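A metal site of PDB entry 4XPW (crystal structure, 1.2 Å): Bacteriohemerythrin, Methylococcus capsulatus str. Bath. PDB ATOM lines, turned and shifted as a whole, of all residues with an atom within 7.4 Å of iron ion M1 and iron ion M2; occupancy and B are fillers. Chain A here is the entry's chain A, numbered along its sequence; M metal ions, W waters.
A ring nitrogen (ND1) of His 58 sits at hydrogen-bond distance from the side-chain amide oxygen (OE1) of Gln 21 (2.7 Å). OE2 of Glu 62 sits close to OH of Tyr 125 (2.7 Å). A ring nitrogen (ND1) of His 81 sits at hydrogen-bond distance from the side-chain carboxylate of Glu 63, at 2.8 Å. A ring nitrogen (ND1) of His 22 lies close to the backbone carbonyl oxygen (O) of Ala 18 (3.2 Å). ND1 of His 77 is in hydrogen-bond range of SD of Met 66 (3.4 Å).
Of the 23 residues printed, 4 come within 4 Å of iron ion M2.
Iron ion M1 is bound by water W2, OD1 of Asp 122, OE1 of Glu 62, NE2 of His 117, NE2 of His 81 and NE2 of His 77. Iron ion M1 has six donor atoms within binding distance.
Iron ion M2 is bound by water W2, 1.9 Å away. Iron ion M2 is bound by the side-chain carboxylate (OD2) of Asp 122. Iron ion M2 is bound by NE2 of His 58, at 2.1 Å. NE2 of His 22 binds iron ion M2, at 2.2 Å. OE2 of Glu 62 is bound to iron ion M2, 2.3 Å away. Iron ion M2 is bound by water W1 (2.4 Å).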
ATOM      1  N   THR A  13       8.755   3.726   7.815  1.00  0.00           N
ATOM      2  CA  THR A  13       8.285   3.318   9.133  1.00  0.00           C
ATOM      3  C   THR A  13       9.406   3.082  10.120  1.00  0.00           C
ATOM      4  O   THR A  13       9.101   2.815  11.293  1.00  0.00           O
ATOM      5  CB  THR A  13       7.488   1.985   9.053  1.00  0.00           C
ATOM      6  OG1 THR A  13       8.414   0.947   8.617  1.00  0.00           O
ATOM      7  CG2 THR A  13       6.295   2.051   8.152  1.00  0.00           C
ATOM      8  N   ALA A  18       9.010  -4.048   6.802  1.00  0.00           N
ATOM      9  CA  ALA A  18       7.739  -3.453   6.437  1.00  0.00           C
ATOM     10  C   ALA A  18       7.954  -2.503   5.278  1.00  0.00           C
ATOM     11  O   ALA A  18       7.163  -2.453   4.330  1.00  0.00           O
ATOM     12  CB  ALA A  18       7.140  -2.726   7.642  1.00  0.00           C
ATOM     13  N   ASP A  19       8.974  -1.664   5.350  1.00  0.00           N
ATOM     14  CA  ASP A  19       9.269  -0.784   4.227  1.00  0.00           C
ATOM     15  C   ASP A  19       9.476  -1.568   2.945  1.00  0.00           C
ATOM     16  O   ASP A  19       9.001  -1.142   1.875  1.00  0.00           O
ATOM     17  CB  ASP A  19      10.557   0.053   4.522  1.00  0.00           C
ATOM     18  CG  ASP A  19      10.304   1.117   5.568  1.00  0.00           C
ATOM     19  OD1 ASP A  19       9.226   1.519   5.925  1.00  0.00           O
ATOM     20  OD2 ASP A  19      11.405   1.580   6.052  1.00  0.00           O
ATOM     21  N   GLN A  21       8.290  -4.581   2.167  1.00  0.00           N
ATOM     22  CA  GLN A  21       7.023  -5.140   1.693  1.00  0.00           C
ATOM     23  C   GLN A  21       6.135  -4.044   1.113  1.00  0.00           C
ATOM     24  O   GLN A  21       5.447  -4.269   0.106  1.00  0.00           O
ATOM     25  CB  GLN A  21       6.304  -5.902   2.830  1.00  0.00           C
ATOM     26  CG  GLN A  21       7.084  -7.140   3.289  1.00  0.00           C
ATOM     27  CD  GLN A  21       6.372  -7.864   4.391  1.00  0.00           C
ATOM     28  OE1 GLN A  21       5.695  -7.345   5.209  1.00  0.00           O
ATOM     29  NE2 GLN A  21       6.580  -9.198   4.428  1.00  0.00           N
ATOM     30  N   HIS A  22       6.157  -2.841   1.695  1.00  0.00           N
ATOM     31  CA  HIS A  22       5.416  -1.720   1.114  1.00  0.00           C
ATOM     32  C   HIS A  22       5.901  -1.384  -0.277  1.00  0.00           C
ATOM     33  O   HIS A  22       5.116  -1.125  -1.191  1.00  0.00           O
ATOM     34  CB  HIS A  22       5.489  -0.491   2.033  1.00  0.00           C
ATOM     35  CG  HIS A  22       4.796  -0.702   3.331  1.00  0.00           C
ATOM     36  ND1 HIS A  22       5.124   0.018   4.462  1.00  0.00           N
ATOM     37  CD2 HIS A  22       3.796  -1.534   3.715  1.00  0.00           C
ATOM     38  CE1 HIS A  22       4.333  -0.340   5.465  1.00  0.00           C
ATOM     39  NE2 HIS A  22       3.521  -1.303   5.051  1.00  0.00           N
ATOM     40  N   ILE A  25       4.441  -3.889  -2.606  1.00  0.00           N
ATOM     41  CA  ILE A  25       3.043  -3.579  -2.841  1.00  0.00           C
ATOM     42  C   ILE A  25       2.909  -2.455  -3.868  1.00  0.00           C
ATOM     43  O   ILE A  25       2.085  -2.554  -4.799  1.00  0.00           O
ATOM     44  CB  ILE A  25       2.343  -3.223  -1.521  1.00  0.00           C
ATOM     45  CG1 ILE A  25       2.164  -4.476  -0.686  1.00  0.00           C
ATOM     46  CG2 ILE A  25       0.955  -2.558  -1.759  1.00  0.00           C
ATOM     47  CD1 ILE A  25       1.757  -4.270   0.761  1.00  0.00           C
ATOM     48  N   HIS A  58       1.766  -9.582   3.721  1.00  0.00           N
ATOM     49  CA  HIS A  58       2.310  -8.383   4.386  1.00  0.00           C
ATOM     50  C   HIS A  58       1.551  -8.156   5.696  1.00  0.00           C
ATOM     51  O   HIS A  58       2.189  -7.902   6.730  1.00  0.00           O
ATOM     52  CB  HIS A  58       2.204  -7.219   3.455  1.00  0.00           C
ATOM     53  CG  HIS A  58       2.436  -5.885   4.183  1.00  0.00           C
ATOM     54  ND1 HIS A  58       3.615  -5.619   4.845  1.00  0.00           N
ATOM     55  CD2 HIS A  58       1.612  -4.818   4.367  1.00  0.00           C
ATOM     56  CE1 HIS A  58       3.465  -4.425   5.432  1.00  0.00           C
ATOM     57  NE2 HIS A  58       2.262  -3.912   5.162  1.00  0.00           N
ATOM     58  N   PHE A  59       0.246  -8.212   5.661  1.00  0.00           N
ATOM     59  CA  PHE A  59      -0.527  -7.987   6.881  1.00  0.00           C
ATOM     60  C   PHE A  59      -0.209  -9.027   7.916  1.00  0.00           C
ATOM     61  O   PHE A  59      -0.049  -8.703   9.130  1.00  0.00           O
ATOM     62  CB  PHE A  59      -2.019  -7.976   6.560  1.00  0.00           C
ATOM     63  CG  PHE A  59      -2.491  -6.795   5.756  1.00  0.00           C
ATOM     64  CD1 PHE A  59      -3.752  -6.850   5.172  1.00  0.00           C
ATOM     65  CD2 PHE A  59      -1.715  -5.631   5.596  1.00  0.00           C
ATOM     66  CE1 PHE A  59      -4.265  -5.779   4.484  1.00  0.00           C
ATOM     67  CE2 PHE A  59      -2.265  -4.556   4.879  1.00  0.00           C
ATOM     68  CZ  PHE A  59      -3.511  -4.615   4.334  1.00  0.00           C
ATOM     69  N   GLU A  62       3.227  -8.061   9.517  1.00  0.00           N
ATOM     70  CA  GLU A  62       3.089  -6.990  10.499  1.00  0.00           C
ATOM     71  C   GLU A  62       2.346  -7.473  11.733  1.00  0.00           C
ATOM     72  O   GLU A  62       2.773  -7.146  12.888  1.00  0.00           O
ATOM     73  CB  GLU A  62       2.232  -5.835   9.958  1.00  0.00           C
ATOM     74  CG  GLU A  62       2.941  -4.960   8.911  1.00  0.00           C
ATOM     75  CD  GLU A  62       2.136  -3.712   8.576  1.00  0.00           C
ATOM     76  OE1 GLU A  62       0.995  -3.624   9.066  1.00  0.00           O
ATOM     77  OE2 GLU A  62       2.682  -2.854   7.816  1.00  0.00           O
ATOM     78  N   GLU A  63       1.311  -8.243  11.582  1.00  0.00           N
ATOM     79  CA  GLU A  63       0.499  -8.706  12.741  1.00  0.00           C
ATOM     80  C   GLU A  63       1.292  -9.601  13.610  1.00  0.00           C
ATOM     81  O   GLU A  63       1.213  -9.510  14.865  1.00  0.00           O
ATOM     82  CB  GLU A  63      -0.765  -9.384  12.237  1.00  0.00           C
ATOM     83  CG  GLU A  63      -1.734  -8.412  11.639  1.00  0.00           C
ATOM     84  CD  GLU A  63      -2.849  -8.976  10.825  1.00  0.00           C
ATOM     85  OE1 GLU A  63      -3.174 -10.216  11.058  1.00  0.00           O
ATOM     86  OE2 GLU A  63      -3.497  -8.316  10.013  1.00  0.00           O
ATOM     87  N   MET A  66       3.716  -7.302  15.577  1.00  0.00           N
ATOM     88  CA  MET A  66       2.966  -6.481  16.559  1.00  0.00           C
ATOM     89  C   MET A  66       2.521  -7.336  17.692  1.00  0.00           C
ATOM     90  O   MET A  66       2.669  -6.955  18.905  1.00  0.00           O
ATOM     91  CB  MET A  66       1.745  -5.814  15.880  1.00  0.00           C
ATOM     92  CG  MET A  66       2.074  -4.619  15.020  1.00  0.00           C
ATOM     93  SD  MET A  66       0.625  -3.741  14.404  1.00  0.00           S
ATOM     94  CE  MET A  66      -0.029  -4.891  13.142  1.00  0.00           C
ATOM     95  N   HIS A  77      -5.245  -2.050  14.723  1.00  0.00           N
ATOM     96  CA  HIS A  77      -4.477  -2.084  13.453  1.00  0.00           C
ATOM     97  C   HIS A  77      -4.963  -3.281  12.675  1.00  0.00           C
ATOM     98  O   HIS A  77      -5.277  -3.165  11.438  1.00  0.00           O
ATOM     99  CB  HIS A  77      -3.021  -2.064  13.802  1.00  0.00           C
ATOM    100  CG  HIS A  77      -2.135  -1.908  12.600  1.00  0.00           C
ATOM    101  ND1 HIS A  77      -0.964  -1.198  12.717  1.00  0.00           N
ATOM    102  CD2 HIS A  77      -2.187  -2.365  11.310  1.00  0.00           C
ATOM    103  CE1 HIS A  77      -0.358  -1.222  11.526  1.00  0.00           C
ATOM    104  NE2 HIS A  77      -1.049  -1.934  10.662  1.00  0.00           N
ATOM    105  N   LYS A  78      -5.001  -4.450  13.286  1.00  0.00           N
ATOM    106  CA  LYS A  78      -5.482  -5.634  12.570  1.00  0.00           C
ATOM    107  C   LYS A  78      -6.847  -5.442  12.081  1.00  0.00           C
ATOM    108  O   LYS A  78      -7.194  -5.972  10.972  1.00  0.00           O
ATOM    109  CB  LYS A  78      -5.389  -6.837  13.495  1.00  0.00           C
ATOM    110  CG  LYS A  78      -5.932  -8.107  12.818  1.00  0.00           C
ATOM    111  CD  LYS A  78      -5.593  -9.343  13.607  1.00  0.00           C
ATOM    112  CE  LYS A  78      -6.019 -10.650  12.992  1.00  0.00           C
ATOM    113  NZ  LYS A  78      -7.429 -10.651  12.807  1.00  0.00           N
ATOM    114  N   GLU A  80      -8.189  -2.810  10.826  1.00  0.00           N
ATOM    115  CA  GLU A  80      -8.073  -2.100   9.530  1.00  0.00           C
ATOM    116  C   GLU A  80      -7.622  -3.047   8.436  1.00  0.00           C
ATOM    117  O   GLU A  80      -8.223  -3.040   7.342  1.00  0.00           O
ATOM    118  CB  GLU A  80      -7.077  -0.922   9.607  1.00  0.00           C
ATOM    119  CG  GLU A  80      -7.348   0.096  10.727  1.00  0.00           C
ATOM    120  CD  GLU A  80      -8.687   0.735  10.706  1.00  0.00           C
ATOM    121  OE1 GLU A  80      -9.404   0.744   9.708  1.00  0.00           O
ATOM    122  OE2 GLU A  80      -9.098   1.291  11.816  1.00  0.00           O
ATOM    123  N   HIS A  81      -6.632  -3.877   8.711  1.00  0.00           N
ATOM    124  CA  HIS A  81      -6.182  -4.888   7.728  1.00  0.00           C
ATOM    125  C   HIS A  81      -7.358  -5.772   7.340  1.00  0.00           C
ATOM    126  O   HIS A  81      -7.616  -6.045   6.128  1.00  0.00           O
ATOM    127  CB  HIS A  81      -5.137  -5.775   8.317  1.00  0.00           C
ATOM    128  CG  HIS A  81      -3.813  -5.108   8.533  1.00  0.00           C
ATOM    129  ND1 HIS A  81      -2.795  -5.767   9.170  1.00  0.00           N
ATOM    130  CD2 HIS A  81      -3.288  -3.888   8.198  1.00  0.00           C
ATOM    131  CE1 HIS A  81      -1.713  -4.985   9.180  1.00  0.00           C
ATOM    132  NE2 HIS A  81      -1.985  -3.822   8.600  1.00  0.00           N
ATOM    133  N   TRP A 113      -6.059   3.678  -0.045  1.00  0.00           N
ATOM    134  CA  TRP A 113      -5.983   2.922   1.207  1.00  0.00           C
ATOM    135  C   TRP A 113      -4.550   2.919   1.745  1.00  0.00           C
ATOM    136  O   TRP A 113      -4.312   3.183   2.946  1.00  0.00           O
ATOM    137  CB  TRP A 113      -6.577   1.522   1.008  1.00  0.00           C
ATOM    138  CG  TRP A 113      -6.765   0.811   2.307  1.00  0.00           C
ATOM    139  CD1 TRP A 113      -7.990   0.721   2.994  1.00  0.00           C
ATOM    140  CD2 TRP A 113      -5.806   0.154   3.109  1.00  0.00           C
ATOM    141  NE1 TRP A 113      -7.799   0.001   4.136  1.00  0.00           N
ATOM    142  CE2 TRP A 113      -6.479  -0.352   4.266  1.00  0.00           C
ATOM    143  CE3 TRP A 113      -4.459  -0.187   2.945  1.00  0.00           C
ATOM    144  CZ2 TRP A 113      -5.838  -1.081   5.259  1.00  0.00           C
ATOM    145  CZ3 TRP A 113      -3.790  -0.910   3.939  1.00  0.00           C
ATOM    146  CH2 TRP A 113      -4.498  -1.354   5.077  1.00  0.00           C
ATOM    147  N   PHE A 114      -3.572   2.546   0.879  1.00  0.00           N
ATOM    148  CA  PHE A 114      -2.200   2.423   1.359  1.00  0.00           C
ATOM    149  C   PHE A 114      -1.600   3.761   1.710  1.00  0.00           C
ATOM    150  O   PHE A 114      -0.824   3.849   2.691  1.00  0.00           O
ATOM    151  CB  PHE A 114      -1.314   1.741   0.293  1.00  0.00           C
ATOM    152  CG  PHE A 114      -1.619   0.272   0.174  1.00  0.00           C
ATOM    153  CD1 PHE A 114      -1.324  -0.560   1.204  1.00  0.00           C
ATOM    154  CD2 PHE A 114      -2.197  -0.297  -0.954  1.00  0.00           C
ATOM    155  CE1 PHE A 114      -1.657  -1.996   1.162  1.00  0.00           C
ATOM    156  CE2 PHE A 114      -2.459  -1.695  -1.002  1.00  0.00           C
ATOM    157  CZ  PHE A 114      -2.281  -2.386   0.085  1.00  0.00           C
ATOM    158  N   HIS A 117      -3.041   4.456   5.078  1.00  0.00           N
ATOM    159  CA  HIS A 117      -2.710   3.489   6.125  1.00  0.00           C
ATOM    160  C   HIS A 117      -1.243   3.566   6.543  1.00  0.00           C
ATOM    161  O   HIS A 117      -0.915   3.481   7.745  1.00  0.00           O
ATOM    162  CB  HIS A 117      -3.014   2.087   5.621  1.00  0.00           C
ATOM    163  CG  HIS A 117      -2.751   1.000   6.640  1.00  0.00           C
ATOM    164  ND1 HIS A 117      -3.705   0.657   7.610  1.00  0.00           N
ATOM    165  CD2 HIS A 117      -1.706   0.180   6.834  1.00  0.00           C
ATOM    166  CE1 HIS A 117      -3.195  -0.333   8.333  1.00  0.00           C
ATOM    167  NE2 HIS A 117      -1.997  -0.683   7.909  1.00  0.00           N
ATOM    168  N   ILE A 118      -0.318   3.673   5.586  1.00  0.00           N
ATOM    169  CA  ILE A 118       1.084   3.545   5.962  1.00  0.00           C
ATOM    170  C   ILE A 118       1.499   4.731   6.883  1.00  0.00           C
ATOM    171  O   ILE A 118       2.077   4.498   7.899  1.00  0.00           O
ATOM    172  CB  ILE A 118       1.955   3.370   4.706  1.00  0.00           C
ATOM    173  CG1 ILE A 118       1.652   1.993   4.095  1.00  0.00           C
ATOM    174  CG2 ILE A 118       3.445   3.469   5.107  1.00  0.00           C
ATOM    175  CD1 ILE A 118       2.234   1.816   2.657  1.00  0.00           C
ATOM    176  N   VAL A 121      -1.144   4.731  10.260  1.00  0.00           N
ATOM    177  CA  VAL A 121      -1.328   3.506  11.008  1.00  0.00           C
ATOM    178  C   VAL A 121      -0.001   2.785  11.158  1.00  0.00           C
ATOM    179  O   VAL A 121       0.476   2.518  12.284  1.00  0.00           O
ATOM    180  CB  VAL A 121      -2.471   2.601  10.442  1.00  0.00           C
ATOM    181  CG1 VAL A 121      -2.737   1.453  11.368  1.00  0.00           C
ATOM    182  CG2 VAL A 121      -3.748   3.423  10.196  1.00  0.00           C
ATOM    183  N   ASP A 122       0.663   2.464  10.017  1.00  0.00           N
ATOM    184  CA  ASP A 122       1.912   1.705  10.113  1.00  0.00           C
ATOM    185  C   ASP A 122       3.015   2.489  10.781  1.00  0.00           C
ATOM    186  O   ASP A 122       3.783   1.946  11.578  1.00  0.00           O
ATOM    187  CB  ASP A 122       2.391   1.200   8.746  1.00  0.00           C
ATOM    188  CG  ASP A 122       1.561   0.091   8.177  1.00  0.00           C
ATOM    189  OD1 ASP A 122       0.788  -0.557   8.928  1.00  0.00           O
ATOM    190  OD2 ASP A 122       1.774  -0.189   6.957  1.00  0.00           O
ATOM    191  N   LYS A 123       3.163   3.783  10.482  1.00  0.00           N
ATOM    192  CA  LYS A 123       4.297   4.488  11.136  1.00  0.00           C
ATOM    193  C   LYS A 123       4.210   4.418  12.629  1.00  0.00           C
ATOM    194  O   LYS A 123       5.271   4.493  13.314  1.00  0.00           O
ATOM    195  CB  LYS A 123       4.338   5.943  10.705  1.00  0.00           C
ATOM    196  CG  LYS A 123       4.912   6.171   9.333  1.00  0.00           C
ATOM    197  CD  LYS A 123       5.029   7.673   8.978  1.00  0.00           C
ATOM    198  CE  LYS A 123       5.556   7.917   7.620  1.00  0.00           C
ATOM    199  NZ  LYS A 123       5.869   9.351   7.440  1.00  0.00           N
ATOM    200  N   TYR A 125       3.800   1.955  14.580  1.00  0.00           N
ATOM    201  CA  TYR A 125       4.495   0.848  15.196  1.00  0.00           C
ATOM    202  C   TYR A 125       5.988   0.935  15.158  1.00  0.00           C
ATOM    203  O   TYR A 125       6.673   0.070  15.631  1.00  0.00           O
ATOM    204  CB  TYR A 125       4.012  -0.500  14.616  1.00  0.00           C
ATOM    205  CG  TYR A 125       4.202  -0.801  13.150  1.00  0.00           C
ATOM    206  CD1 TYR A 125       5.433  -0.539  12.492  1.00  0.00           C
ATOM    207  CD2 TYR A 125       3.150  -1.321  12.422  1.00  0.00           C
ATOM    208  CE1 TYR A 125       5.564  -0.802  11.116  1.00  0.00           C
ATOM    209  CE2 TYR A 125       3.295  -1.584  11.056  1.00  0.00           C
ATOM    210  CZ  TYR A 125       4.460  -1.282  10.426  1.00  0.00           C
ATOM    211  OH  TYR A 125       4.641  -1.444   9.034  1.00  0.00           O
HETATM  212 FE    FE M   1      -0.544  -2.190   8.514  1.00  0.00          FE
HETATM  213 FE    FE M   2       1.657  -2.020   5.981  1.00  0.00          FE
HETATM  214  O   HOH W   1       0.433  -1.370   3.991  1.00  0.00           O
HETATM  215  O   HOH W   2      -0.019  -2.603   6.714  1.00  0.00           O
